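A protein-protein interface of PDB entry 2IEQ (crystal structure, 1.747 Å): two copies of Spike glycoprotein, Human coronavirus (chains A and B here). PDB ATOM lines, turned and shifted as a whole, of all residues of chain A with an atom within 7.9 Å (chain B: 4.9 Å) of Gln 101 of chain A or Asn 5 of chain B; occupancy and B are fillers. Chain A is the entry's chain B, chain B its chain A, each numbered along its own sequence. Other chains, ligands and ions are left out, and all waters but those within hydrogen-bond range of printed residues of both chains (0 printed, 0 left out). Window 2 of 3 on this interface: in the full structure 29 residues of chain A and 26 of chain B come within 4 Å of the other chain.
Positions printed for both chains: 6 and 7.
Of the 9 pairs that touch across the chains among the printed residues, none has its exchanged pair printed and touching as well.
Hydrophobic or aromatic side chains of chain A within 4 Å of the printed part of chain B: Phe 10, Leu 95, Leu 98 and Ile 102.
Hydrophobic or aromatic side chains of chain B that line the printed part of chain A: Ala 8.
Along chain B the printed residues that touch a printed residue of chain A span positions 5 to 9.
Among the printed residues, no Asp or Glu carboxylate lies within 4 Å of a Lys or Arg side-chain nitrogen of the other chain.
Gln 96 of chain A touches none of the printed residues of chain B.
Of the printed residues of chain B, Leu 98 of chain A touches Asn 5 (3.8 Å), Ala 8 (3.6 Å) and Ser 9 (3.2 Å).
Printed residues of chain B within 4 Å of Gln 101 of chain A: Asn 5 (3.4 Å).
Printed residues of chain B within 4 Å of Ile 102 of chain A: Asn 5 (3.8 Å) and Ser 9 (3.9 Å).
Asn 5 of chain B touches just these residues of chain A: Leu 98, Gln 101 and Ile 102.
The nearest printed residue of chain B that does not touch Gln 101 of chain A is Ala 2 of chain B (6.7 Å).
The nearest printed residue of chain A that does not touch Ala 8 of chain B is Leu 95 of chain A (5.6 Å).
The side-chain amide nitrogen (ND2) of Asn 5 of chain B lies close to the side-chain amide nitrogen (NE2) of Gln 101 of chain A (3.4 Å).
Among the printed residues, pairs that only touch across the chains: Phe 10 of chain A with Ile 6 of chain B (3.8 Å), Phe 10 of chain A with Ser 9 of chain B (3.6 Å), Leu 95 of chain A with Ser 9 of chain B (3.7 Å), Leu 98 of chain A with Asn 5 of chain B (3.8 Å), Leu 98 of chain A with Ala 8 of chain B (3.6 Å), Leu 98 of chain A with Ser 9 of chain B (3.2 Å), Ile 102 of chain A with Asn 5 of chain B (3.8 Å) and Ile 102 of chain A with Ser 9 of chain B (3.9 Å).
The side-chain hydroxyl of Ser 9 of chain B sits at hydrogen-bond distance from the backbone carbonyl oxygen of Asn 5 of chain B (2.6 Å).
O of Gln 101 of chain A lies within hydrogen-bond range of OG of Ser 104 of chain A (3.1 Å).
O of Gln 101 of chain A sits at hydrogen-bond distance from OG1 of Thr 105 of chain A, at 2.5 Å.
The side-chain hydroxyl (OG1) of Thr 105 of chain A lies within hydrogen-bond range of the backbone carbonyl oxygen (O) of Ile 102 of chain A (3.2 Å).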
ATOM      1  N   ILE A   6      27.347  -5.185   1.102  1.00  0.00           N
ATOM      2  CA  ILE A   6      26.322  -4.553   0.267  1.00  0.00           C
ATOM      3  C   ILE A   6      25.627  -3.397   1.023  1.00  0.00           C
ATOM      4  O   ILE A   6      25.465  -2.284   0.505  1.00  0.00           O
ATOM      5  CB  ILE A   6      25.324  -5.605  -0.316  1.00  0.00           C
ATOM      6  CG1 ILE A   6      26.054  -6.537  -1.291  1.00  0.00           C
ATOM      7  CG2 ILE A   6      24.208  -4.930  -1.106  1.00  0.00           C
ATOM      8  CD1 ILE A   6      25.266  -7.926  -1.454  1.00  0.00           C
ATOM      9  N   VAL A   7      25.255  -3.648   2.268  1.00  0.00           N
ATOM     10  CA  VAL A   7      24.649  -2.588   3.096  1.00  0.00           C
ATOM     11  C   VAL A   7      25.642  -1.432   3.280  1.00  0.00           C
ATOM     12  O   VAL A   7      25.291  -0.241   3.042  1.00  0.00           O
ATOM     13  CB  VAL A   7      24.121  -3.116   4.410  1.00  0.00           C
ATOM     14  CG1 VAL A   7      23.621  -1.970   5.273  1.00  0.00           C
ATOM     15  CG2 VAL A   7      22.961  -4.086   4.126  1.00  0.00           C
ATOM     16  N   PHE A  10      25.880   0.568  -0.043  1.00  0.00           N
ATOM     17  CA  PHE A  10      24.753   1.508  -0.262  1.00  0.00           C
ATOM     18  C   PHE A  10      24.864   2.718   0.705  1.00  0.00           C
ATOM     19  O   PHE A  10      24.569   3.824   0.333  1.00  0.00           O
ATOM     20  CB  PHE A  10      23.403   0.817  -0.100  1.00  0.00           C
ATOM     21  CG  PHE A  10      22.983   0.027  -1.296  1.00  0.00           C
ATOM     22  CD1 PHE A  10      22.829   0.652  -2.569  1.00  0.00           C
ATOM     23  CD2 PHE A  10      22.667  -1.290  -1.171  1.00  0.00           C
ATOM     24  CE1 PHE A  10      22.440  -0.090  -3.681  1.00  0.00           C
ATOM     25  CE2 PHE A  10      22.223  -2.012  -2.275  1.00  0.00           C
ATOM     26  CZ  PHE A  10      22.145  -1.414  -3.534  1.00  0.00           C
ATOM     27  N   GLU A  94      14.657   8.030   1.111  1.00  0.00           N
ATOM     28  CA  GLU A  94      14.161   6.790   0.461  1.00  0.00           C
ATOM     29  C   GLU A  94      15.162   5.670   0.472  1.00  0.00           C
ATOM     30  O   GLU A  94      14.839   4.516   0.900  1.00  0.00           O
ATOM     31  CB  GLU A  94      13.719   7.122  -0.965  1.00  0.00           C
ATOM     32  CG  GLU A  94      12.409   7.908  -0.994  1.00  0.00           C
ATOM     33  CD  GLU A  94      12.106   8.597  -2.341  1.00  0.00           C
ATOM     34  OE1 GLU A  94      12.881   8.418  -3.326  1.00  0.00           O
ATOM     35  OE2 GLU A  94      11.098   9.340  -2.415  1.00  0.00           O
ATOM     36  N   LEU A  95      16.390   5.992   0.052  1.00  0.00           N
ATOM     37  CA  LEU A  95      17.482   5.027   0.023  1.00  0.00           C
ATOM     38  C   LEU A  95      17.834   4.592   1.431  1.00  0.00           C
ATOM     39  O   LEU A  95      18.139   3.418   1.645  1.00  0.00           O
ATOM     40  CB  LEU A  95      18.741   5.607  -0.626  1.00  0.00           C
ATOM     41  CG  LEU A  95      19.925   4.626  -0.777  1.00  0.00           C
ATOM     42  CD1 LEU A  95      19.501   3.278  -1.491  1.00  0.00           C
ATOM     43  CD2 LEU A  95      21.053   5.260  -1.603  1.00  0.00           C
ATOM     44  N   GLN A  96      17.845   5.518   2.399  1.00  0.00           N
ATOM     45  CA  GLN A  96      18.018   5.053   3.813  1.00  0.00           C
ATOM     46  C   GLN A  96      16.918   4.066   4.228  1.00  0.00           C
ATOM     47  O   GLN A  96      17.219   3.043   4.878  1.00  0.00           O
ATOM     48  CB  GLN A  96      18.098   6.228   4.814  1.00  0.00           C
ATOM     49  CG  GLN A  96      18.301   5.786   6.241  1.00  0.00           C
ATOM     50  CD  GLN A  96      19.686   5.181   6.402  1.00  0.00           C
ATOM     51  OE1 GLN A  96      20.677   5.872   6.177  1.00  0.00           O
ATOM     52  NE2 GLN A  96      19.763   3.876   6.753  1.00  0.00           N
ATOM     53  N   GLY A  97      15.673   4.323   3.849  1.00  0.00           N
ATOM     54  CA  GLY A  97      14.559   3.389   4.154  1.00  0.00           C
ATOM     55  C   GLY A  97      14.780   1.991   3.543  1.00  0.00           C
ATOM     56  O   GLY A  97      14.526   0.950   4.177  1.00  0.00           O
ATOM     57  N   LEU A  98      15.263   1.963   2.315  1.00  0.00           N
ATOM     58  CA  LEU A  98      15.515   0.705   1.628  1.00  0.00           C
ATOM     59  C   LEU A  98      16.691  -0.024   2.288  1.00  0.00           C
ATOM     60  O   LEU A  98      16.669  -1.253   2.438  1.00  0.00           O
ATOM     61  CB  LEU A  98      15.790   0.995   0.148  1.00  0.00           C
ATOM     62  CG  LEU A  98      14.538   1.296  -0.685  1.00  0.00           C
ATOM     63  CD1 LEU A  98      14.907   1.831  -2.023  1.00  0.00           C
ATOM     64  CD2 LEU A  98      13.784  -0.047  -0.832  1.00  0.00           C
ATOM     65  N   ILE A  99      17.749   0.728   2.665  1.00  0.00           N
ATOM     66  CA  ILE A  99      18.863   0.167   3.449  1.00  0.00           C
ATOM     67  C   ILE A  99      18.288  -0.439   4.751  1.00  0.00           C
ATOM     68  O   ILE A  99      18.643  -1.546   5.160  1.00  0.00           O
ATOM     69  CB  ILE A  99      19.947   1.203   3.776  1.00  0.00           C
ATOM     70  CG1 ILE A  99      20.677   1.654   2.485  1.00  0.00           C
ATOM     71  CG2 ILE A  99      21.020   0.625   4.676  1.00  0.00           C
ATOM     72  CD1 ILE A  99      21.689   2.849   2.703  1.00  0.00           C
ATOM     73  N   ASP A 100      17.367   0.280   5.396  1.00  0.00           N
ATOM     74  CA  ASP A 100      16.737  -0.286   6.612  1.00  0.00           C
ATOM     75  C   ASP A 100      16.002  -1.586   6.301  1.00  0.00           C
ATOM     76  O   ASP A 100      15.995  -2.507   7.110  1.00  0.00           O
ATOM     77  CB  ASP A 100      15.762   0.710   7.232  1.00  0.00           C
ATOM     78  CG  ASP A 100      16.445   1.980   7.742  1.00  0.00           C
ATOM     79  OD1 ASP A 100      17.673   1.979   8.018  1.00  0.00           O
ATOM     80  OD2 ASP A 100      15.693   3.006   7.871  1.00  0.00           O
ATOM     81  N   GLN A 101      15.406  -1.684   5.106  1.00  0.00           N
ATOM     82  CA  GLN A 101      14.753  -2.941   4.729  1.00  0.00           C
ATOM     83  C   GLN A 101      15.715  -4.103   4.504  1.00  0.00           C
ATOM     84  O   GLN A 101      15.367  -5.274   4.854  1.00  0.00           O
ATOM     85  CB  GLN A 101      13.880  -2.764   3.518  1.00  0.00           C
ATOM     86  CG  GLN A 101      12.667  -1.900   3.754  1.00  0.00           C
ATOM     87  CD  GLN A 101      11.637  -2.105   2.670  1.00  0.00           C
ATOM     88  OE1 GLN A 101      11.261  -1.166   1.959  1.00  0.00           O
ATOM     89  NE2 GLN A 101      11.184  -3.360   2.511  1.00  0.00           N
ATOM     90  N   ILE A 102      16.888  -3.824   3.909  1.00  0.00           N
ATOM     91  CA  ILE A 102      17.865  -4.884   3.627  1.00  0.00           C
ATOM     92  C   ILE A 102      18.332  -5.347   4.975  1.00  0.00           C
ATOM     93  O   ILE A 102      18.212  -6.523   5.302  1.00  0.00           O
ATOM     94  CB  ILE A 102      19.075  -4.398   2.806  1.00  0.00           C
ATOM     95  CG1 ILE A 102      18.630  -3.982   1.390  1.00  0.00           C
ATOM     96  CG2 ILE A 102      20.181  -5.466   2.810  1.00  0.00           C
ATOM     97  CD1 ILE A 102      19.694  -3.213   0.626  1.00  0.00           C
ATOM     98  N   ASN A 103      18.811  -4.393   5.773  1.00  0.00           N
ATOM     99  CA  ASN A 103      19.245  -4.634   7.145  1.00  0.00           C
ATOM    100  C   ASN A 103      18.337  -5.497   7.988  1.00  0.00           C
ATOM    101  O   ASN A 103      18.803  -6.230   8.856  1.00  0.00           O
ATOM    102  CB  ASN A 103      19.378  -3.312   7.854  1.00  0.00           C
ATOM    103  CG  ASN A 103      20.756  -2.798   7.831  1.00  0.00           C
ATOM    104  OD1 ASN A 103      20.982  -1.589   7.957  1.00  0.00           O
ATOM    105  ND2 ASN A 103      21.714  -3.693   7.680  1.00  0.00           N
ATOM    106  N   SER A 104      17.035  -5.400   7.753  1.00  0.00           N
ATOM    107  CA  SER A 104      16.096  -6.174   8.529  1.00  0.00           C
ATOM    108  C   SER A 104      15.707  -7.509   7.883  1.00  0.00           C
ATOM    109  O   SER A 104      15.178  -8.374   8.584  1.00  0.00           O
ATOM    110  CB  SER A 104      14.851  -5.342   8.827  1.00  0.00           C
ATOM    111  OG  SER A 104      14.122  -5.085   7.643  1.00  0.00           O
ATOM    112  N   THR A 105      15.966  -7.697   6.585  1.00  0.00           N
ATOM    113  CA  THR A 105      15.611  -8.972   5.911  1.00  0.00           C
ATOM    114  C   THR A 105      16.514 -10.139   6.325  1.00  0.00           C
ATOM    115  O   THR A 105      17.308 -10.043   7.270  1.00  0.00           O
ATOM    116  CB  THR A 105      15.579  -8.899   4.330  1.00  0.00           C
ATOM    117  OG1 THR A 105      15.512  -7.543   3.861  1.00  0.00           O
ATOM    118  CG2 THR A 105      14.390  -9.680   3.770  1.00  0.00           C
ATOM    119  N   ALA B   2      15.385 -10.592  -0.564  1.00  0.00           N
ATOM    120  CA  ALA B   2      16.225  -9.372  -0.382  1.00  0.00           C
ATOM    121  C   ALA B   2      16.549  -8.689  -1.724  1.00  0.00           C
ATOM    122  O   ALA B   2      16.812  -7.471  -1.757  1.00  0.00           O
ATOM    123  CB  ALA B   2      17.503  -9.717   0.390  1.00  0.00           C
ATOM    124  N   ILE B   3      16.499  -9.471  -2.816  1.00  0.00           N
ATOM    125  CA  ILE B   3      16.818  -9.006  -4.170  1.00  0.00           C
ATOM    126  C   ILE B   3      15.999  -7.790  -4.535  1.00  0.00           C
ATOM    127  O   ILE B   3      16.524  -6.834  -5.108  1.00  0.00           O
ATOM    128  CB  ILE B   3      16.623 -10.122  -5.271  1.00  0.00           C
ATOM    129  CG1 ILE B   3      17.881 -10.976  -5.406  1.00  0.00           C
ATOM    130  CG2 ILE B   3      16.266  -9.524  -6.675  1.00  0.00           C
ATOM    131  CD1 ILE B   3      18.979 -10.367  -6.303  1.00  0.00           C
ATOM    132  N   ASN B   4      14.711  -7.826  -4.201  1.00  0.00           N
ATOM    133  CA  ASN B   4      13.839  -6.724  -4.548  1.00  0.00           C
ATOM    134  C   ASN B   4      14.357  -5.421  -3.970  1.00  0.00           C
ATOM    135  O   ASN B   4      14.331  -4.420  -4.656  1.00  0.00           O
ATOM    136  CB  ASN B   4      12.424  -6.964  -4.064  1.00  0.00           C
ATOM    137  CG  ASN B   4      11.810  -8.205  -4.671  1.00  0.00           C
ATOM    138  OD1 ASN B   4      11.868  -8.423  -5.893  1.00  0.00           O
ATOM    139  ND2 ASN B   4      11.199  -9.028  -3.819  1.00  0.00           N
ATOM    140  N   ASN B   5      14.823  -5.448  -2.723  1.00  0.00           N
ATOM    141  CA  ASN B   5      15.273  -4.225  -2.063  1.00  0.00           C
ATOM    142  C   ASN B   5      16.633  -3.751  -2.563  1.00  0.00           C
ATOM    143  O   ASN B   5      16.902  -2.552  -2.538  1.00  0.00           O
ATOM    144  CB  ASN B   5      15.334  -4.409  -0.545  1.00  0.00           C
ATOM    145  CG  ASN B   5      13.960  -4.567   0.066  1.00  0.00           C
ATOM    146  OD1 ASN B   5      13.724  -5.498   0.811  1.00  0.00           O
ATOM    147  ND2 ASN B   5      13.034  -3.690  -0.307  1.00  0.00           N
ATOM    148  N   ILE B   6      17.501  -4.699  -2.944  1.00  0.00           N
ATOM    149  CA  ILE B   6      18.737  -4.365  -3.677  1.00  0.00           C
ATOM    150  C   ILE B   6      18.437  -3.692  -5.015  1.00  0.00           C
ATOM    151  O   ILE B   6      19.047  -2.669  -5.344  1.00  0.00           O
ATOM    152  CB  ILE B   6      19.650  -5.632  -3.850  1.00  0.00           C
ATOM    153  CG1 ILE B   6      20.261  -5.985  -2.497  1.00  0.00           C
ATOM    154  CG2 ILE B   6      20.774  -5.398  -4.919  1.00  0.00           C
ATOM    155  CD1 ILE B   6      20.690  -7.419  -2.392  1.00  0.00           C
ATOM    156  N   VAL B   7      17.529  -4.285  -5.793  1.00  0.00           N
ATOM    157  CA  VAL B   7      17.071  -3.666  -7.023  1.00  0.00           C
ATOM    158  C   VAL B   7      16.488  -2.275  -6.789  1.00  0.00           C
ATOM    159  O   VAL B   7      16.837  -1.327  -7.501  1.00  0.00           O
ATOM    160  CB  VAL B   7      16.049  -4.557  -7.772  1.00  0.00           C
ATOM    161  CG1 VAL B   7      15.266  -3.740  -8.810  1.00  0.00           C
ATOM    162  CG2 VAL B   7      16.796  -5.691  -8.402  1.00  0.00           C
ATOM    163  N   ALA B   8      15.626  -2.137  -5.788  1.00  0.00           N
ATOM    164  CA  ALA B   8      14.984  -0.860  -5.539  1.00  0.00           C
ATOM    165  C   ALA B   8      16.041   0.171  -5.107  1.00  0.00           C
ATOM    166  O   ALA B   8      15.956   1.376  -5.445  1.00  0.00           O
ATOM    167  CB  ALA B   8      13.936  -1.029  -4.464  1.00  0.00           C
ATOM    168  N   SER B   9      17.028  -0.301  -4.383  1.00  0.00           N
ATOM    169  CA  SER B   9      18.067   0.607  -3.870  1.00  0.00           C
ATOM    170  C   SER B   9      18.944   1.098  -5.041  1.00  0.00           C
ATOM    171  O   SER B   9      19.223   2.293  -5.152  1.00  0.00           O
ATOM    172  CB  SER B   9      18.888  -0.098  -2.774  1.00  0.00           C
ATOM    173  OG  SER B   9      18.095  -0.423  -1.585  1.00  0.00           O
